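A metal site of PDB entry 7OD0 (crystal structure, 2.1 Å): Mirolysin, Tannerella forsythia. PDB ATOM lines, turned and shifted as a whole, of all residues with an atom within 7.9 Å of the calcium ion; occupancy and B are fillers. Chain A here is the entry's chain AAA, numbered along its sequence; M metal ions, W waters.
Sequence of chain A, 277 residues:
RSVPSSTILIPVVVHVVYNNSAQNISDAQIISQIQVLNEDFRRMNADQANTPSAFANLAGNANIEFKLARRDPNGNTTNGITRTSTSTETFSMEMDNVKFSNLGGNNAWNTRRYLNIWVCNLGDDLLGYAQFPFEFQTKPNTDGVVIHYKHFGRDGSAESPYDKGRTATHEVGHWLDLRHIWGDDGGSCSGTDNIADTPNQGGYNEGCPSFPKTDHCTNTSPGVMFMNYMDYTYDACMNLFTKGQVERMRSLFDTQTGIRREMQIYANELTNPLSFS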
ATOM      1  N   HIS A 180      28.504 -28.767  13.780  1.00  0.00           N
ATOM      2  CA  HIS A 180      27.183 -29.224  14.265  1.00  0.00           C
ATOM      3  C   HIS A 180      27.027 -28.862  15.746  1.00  0.00           C
ATOM      4  O   HIS A 180      27.945 -29.168  16.558  1.00  0.00           O
ATOM      5  CB  HIS A 180      26.990 -30.735  14.031  1.00  0.00           C
ATOM      6  CG  HIS A 180      26.899 -31.073  12.585  1.00  0.00           C
ATOM      7  ND1 HIS A 180      27.401 -32.229  12.069  1.00  0.00           N
ATOM      8  CD2 HIS A 180      26.326 -30.403  11.553  1.00  0.00           C
ATOM      9  CE1 HIS A 180      27.154 -32.285  10.782  1.00  0.00           C
ATOM     10  NE2 HIS A 180      26.491 -31.181  10.429  1.00  0.00           N
ATOM     11  N   ILE A 181      25.885 -28.246  16.067  1.00  0.00           N
ATOM     12  CA  ILE A 181      25.605 -27.659  17.397  1.00  0.00           C
ATOM     13  C   ILE A 181      25.659 -28.748  18.466  1.00  0.00           C
ATOM     14  O   ILE A 181      25.961 -28.390  19.621  1.00  0.00           O
ATOM     15  CB  ILE A 181      24.250 -26.916  17.387  1.00  0.00           C
ATOM     16  CG1 ILE A 181      24.037 -26.118  18.674  1.00  0.00           C
ATOM     17  CG2 ILE A 181      23.108 -27.880  17.115  1.00  0.00           C
ATOM     18  CD1 ILE A 181      22.910 -25.145  18.582  1.00  0.00           C
ATOM     19  N   TRP A 182      25.377 -30.016  18.122  1.00  0.00           N
ATOM     20  CA  TRP A 182      25.328 -31.140  19.100  1.00  0.00           C
ATOM     21  C   TRP A 182      26.742 -31.752  19.281  1.00  0.00           C
ATOM     22  O   TRP A 182      26.921 -32.583  20.186  1.00  0.00           O
ATOM     23  CB  TRP A 182      24.268 -32.178  18.668  1.00  0.00           C
ATOM     24  CG  TRP A 182      24.629 -32.965  17.456  1.00  0.00           C
ATOM     25  CD1 TRP A 182      25.285 -34.154  17.452  1.00  0.00           C
ATOM     26  CD2 TRP A 182      24.359 -32.657  16.084  1.00  0.00           C
ATOM     27  NE1 TRP A 182      25.477 -34.596  16.165  1.00  0.00           N
ATOM     28  CE2 TRP A 182      24.911 -33.695  15.306  1.00  0.00           C
ATOM     29  CE3 TRP A 182      23.703 -31.615  15.416  1.00  0.00           C
ATOM     30  CZ2 TRP A 182      24.841 -33.698  13.905  1.00  0.00           C
ATOM     31  CZ3 TRP A 182      23.646 -31.619  14.035  1.00  0.00           C
ATOM     32  CH2 TRP A 182      24.187 -32.663  13.297  1.00  0.00           C
ATOM     33  N   GLY A 183      27.727 -31.358  18.468  1.00  0.00           N
ATOM     34  CA  GLY A 183      29.127 -31.755  18.678  1.00  0.00           C
ATOM     35  C   GLY A 183      29.518 -33.053  17.990  1.00  0.00           C
ATOM     36  O   GLY A 183      30.592 -33.604  18.332  1.00  0.00           O
ATOM     37  N   GLY A 191      30.938 -34.240  23.331  1.00  0.00           N
ATOM     38  CA  GLY A 191      31.342 -33.407  22.171  1.00  0.00           C
ATOM     39  C   GLY A 191      30.939 -31.947  22.348  1.00  0.00           C
ATOM     40  O   GLY A 191      30.015 -31.650  23.133  1.00  0.00           O
ATOM     41  N   THR A 192      31.592 -31.050  21.621  1.00  0.00           N
ATOM     42  CA  THR A 192      31.349 -29.593  21.665  1.00  0.00           C
ATOM     43  C   THR A 192      31.425 -29.020  20.250  1.00  0.00           C
ATOM     44  O   THR A 192      32.187 -29.545  19.466  1.00  0.00           O
ATOM     45  CB  THR A 192      32.355 -28.902  22.599  1.00  0.00           C
ATOM     46  OG1 THR A 192      32.054 -27.505  22.560  1.00  0.00           O
ATOM     47  CG2 THR A 192      33.801 -29.082  22.207  1.00  0.00           C
ATOM     48  N   ASP A 193      30.669 -27.964  19.969  1.00  0.00           N
ATOM     49  CA  ASP A 193      30.799 -27.152  18.736  1.00  0.00           C
ATOM     50  C   ASP A 193      31.773 -25.988  18.995  1.00  0.00           C
ATOM     51  O   ASP A 193      31.988 -25.177  18.077  1.00  0.00           O
ATOM     52  CB  ASP A 193      29.420 -26.683  18.254  1.00  0.00           C
ATOM     53  CG  ASP A 193      28.725 -25.713  19.188  1.00  0.00           C
ATOM     54  OD1 ASP A 193      29.197 -25.571  20.340  1.00  0.00           O
ATOM     55  OD2 ASP A 193      27.738 -25.099  18.751  1.00  0.00           O
ATOM     56  N   ASN A 194      32.368 -25.950  20.191  1.00  0.00           N
ATOM     57  CA  ASN A 194      33.326 -24.917  20.654  1.00  0.00           C
ATOM     58  C   ASN A 194      32.660 -23.540  20.557  1.00  0.00           C
ATOM     59  O   ASN A 194      33.350 -22.565  20.167  1.00  0.00           O
ATOM     60  CB  ASN A 194      34.650 -24.930  19.880  1.00  0.00           C
ATOM     61  CG  ASN A 194      35.402 -26.224  20.025  1.00  0.00           C
ATOM     62  OD1 ASN A 194      35.167 -27.174  19.290  1.00  0.00           O
ATOM     63  ND2 ASN A 194      36.331 -26.279  20.945  1.00  0.00           N
ATOM     64  N   ILE A 195      31.379 -23.473  20.879  1.00  0.00           N
ATOM     65  CA  ILE A 195      30.617 -22.195  20.934  1.00  0.00           C
ATOM     66  C   ILE A 195      29.956 -22.107  22.313  1.00  0.00           C
ATOM     67  O   ILE A 195      29.092 -22.955  22.635  1.00  0.00           O
ATOM     68  CB  ILE A 195      29.601 -22.061  19.774  1.00  0.00           C
ATOM     69  CG1 ILE A 195      30.258 -22.255  18.405  1.00  0.00           C
ATOM     70  CG2 ILE A 195      28.878 -20.733  19.871  1.00  0.00           C
ATOM     71  CD1 ILE A 195      31.149 -21.113  17.956  1.00  0.00           C
ATOM     72  N   ALA A 196      30.344 -21.078  23.077  1.00  0.00           N
ATOM     73  CA  ALA A 196      29.933 -20.846  24.471  1.00  0.00           C
ATOM     74  C   ALA A 196      28.421 -20.598  24.521  1.00  0.00           C
ATOM     75  O   ALA A 196      27.794 -21.089  25.495  1.00  0.00           O
ATOM     76  CB  ALA A 196      30.722 -19.679  25.034  1.00  0.00           C
ATOM     77  N   ASP A 197      27.836 -19.895  23.543  1.00  0.00           N
ATOM     78  CA  ASP A 197      26.425 -19.414  23.653  1.00  0.00           C
ATOM     79  C   ASP A 197      25.445 -20.383  22.974  1.00  0.00           C
ATOM     80  O   ASP A 197      24.238 -20.040  22.908  1.00  0.00           O
ATOM     81  CB  ASP A 197      26.302 -17.966  23.176  1.00  0.00           C
ATOM     82  CG  ASP A 197      26.684 -17.735  21.727  1.00  0.00           C
ATOM     83  OD1 ASP A 197      26.939 -18.728  21.008  1.00  0.00           O
ATOM     84  OD2 ASP A 197      26.690 -16.564  21.322  1.00  0.00           O
ATOM     85  N   THR A 198      25.896 -21.542  22.486  1.00  0.00           N
ATOM     86  CA  THR A 198      25.000 -22.646  22.025  1.00  0.00           C
ATOM     87  C   THR A 198      24.899 -23.664  23.156  1.00  0.00           C
ATOM     88  O   THR A 198      25.897 -24.272  23.553  1.00  0.00           O
ATOM     89  CB  THR A 198      25.452 -23.328  20.724  1.00  0.00           C
ATOM     90  OG1 THR A 198      26.808 -23.762  20.843  1.00  0.00           O
ATOM     91  CG2 THR A 198      25.324 -22.418  19.519  1.00  0.00           C
ATOM     92  N   PRO A 199      23.691 -23.914  23.700  1.00  0.00           N
ATOM     93  CA  PRO A 199      23.520 -24.833  24.820  1.00  0.00           C
ATOM     94  C   PRO A 199      24.038 -26.230  24.466  1.00  0.00           C
ATOM     95  O   PRO A 199      23.895 -26.632  23.312  1.00  0.00           O
ATOM     96  CB  PRO A 199      21.999 -24.903  25.039  1.00  0.00           C
ATOM     97  CG  PRO A 199      21.454 -23.660  24.376  1.00  0.00           C
ATOM     98  CD  PRO A 199      22.414 -23.330  23.263  1.00  0.00           C
ATOM     99  N   ASN A 200      24.630 -26.921  25.440  1.00  0.00           N
ATOM    100  CA  ASN A 200      25.129 -28.299  25.242  1.00  0.00           C
ATOM    101  C   ASN A 200      23.933 -29.136  24.780  1.00  0.00           C
ATOM    102  O   ASN A 200      22.796 -28.903  25.279  1.00  0.00           O
ATOM    103  CB  ASN A 200      25.811 -28.862  26.494  1.00  0.00           C
ATOM    104  CG  ASN A 200      26.595 -30.123  26.211  1.00  0.00           C
ATOM    105  OD1 ASN A 200      26.984 -30.348  25.067  1.00  0.00           O
ATOM    106  ND2 ASN A 200      26.880 -30.926  27.220  1.00  0.00           N
ATOM    107  N   GLN A 201      24.142 -30.070  23.866  1.00  0.00           N
ATOM    108  CA  GLN A 201      23.021 -30.777  23.200  1.00  0.00           C
ATOM    109  C   GLN A 201      23.459 -32.209  22.905  1.00  0.00           C
ATOM    110  O   GLN A 201      24.606 -32.374  22.424  1.00  0.00           O
ATOM    111  CB  GLN A 201      22.610 -29.972  21.960  1.00  0.00           C
ATOM    112  CG  GLN A 201      21.685 -30.693  21.006  1.00  0.00           C
ATOM    113  CD  GLN A 201      21.220 -29.838  19.849  1.00  0.00           C
ATOM    114  OE1 GLN A 201      21.173 -28.599  19.907  1.00  0.00           O
ATOM    115  NE2 GLN A 201      20.877 -30.512  18.780  1.00  0.00           N
ATOM    116  N   THR A 242      24.286 -17.783  16.460  1.00  0.00           N
ATOM    117  CA  THR A 242      24.609 -17.052  17.698  1.00  0.00           C
ATOM    118  C   THR A 242      25.713 -16.017  17.424  1.00  0.00           C
ATOM    119  O   THR A 242      26.423 -16.127  16.392  1.00  0.00           O
ATOM    120  CB  THR A 242      25.016 -17.960  18.849  1.00  0.00           C
ATOM    121  OG1 THR A 242      26.283 -18.528  18.539  1.00  0.00           O
ATOM    122  CG2 THR A 242      23.977 -19.033  19.151  1.00  0.00           C
ATOM    123  N   GLN A 245      28.864 -17.933  17.230  1.00  0.00           N
ATOM    124  CA  GLN A 245      29.069 -18.511  15.867  1.00  0.00           C
ATOM    125  C   GLN A 245      29.551 -17.410  14.914  1.00  0.00           C
ATOM    126  O   GLN A 245      30.501 -17.656  14.126  1.00  0.00           O
ATOM    127  CB  GLN A 245      27.777 -19.158  15.359  1.00  0.00           C
ATOM    128  CG  GLN A 245      27.407 -20.442  16.084  1.00  0.00           C
ATOM    129  CD  GLN A 245      26.076 -20.991  15.648  1.00  0.00           C
ATOM    130  OE1 GLN A 245      25.114 -20.234  15.464  1.00  0.00           O
ATOM    131  NE2 GLN A 245      26.017 -22.306  15.421  1.00  0.00           N
HETATM  132 CA    CA M   1      27.961 -25.050  22.356  1.00  0.00          CA
HETATM  133  O   HOH W   1      30.622 -25.449  23.373  1.00  0.00           O
HETATM  134  O   HOH W   2      26.143 -26.369  21.619  1.00  0.00           O
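Within 4 Å of the calcium ion: Asp 193, Ile 195 and Thr 198.
Water W2 lies within hydrogen-bond range of O of Pro 199 (2.8 Å) and O of Ile 181 (2.8 Å).
Water W1 bridges OG1 of Thr 192 (2.6 Å) and N of Ile 195 (3.3 Å).
The calcium ion is bound by OG1 of Thr 198 (2.3 Å), water W2 (2.4 Å), O of Ile 195 (2.4 Å), OD1 of Asp 193 (2.4 Å), O of Thr 198 (2.5 Å) and water W1 (2.9 Å).
The calcium ion has six donor atoms within binding distance.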
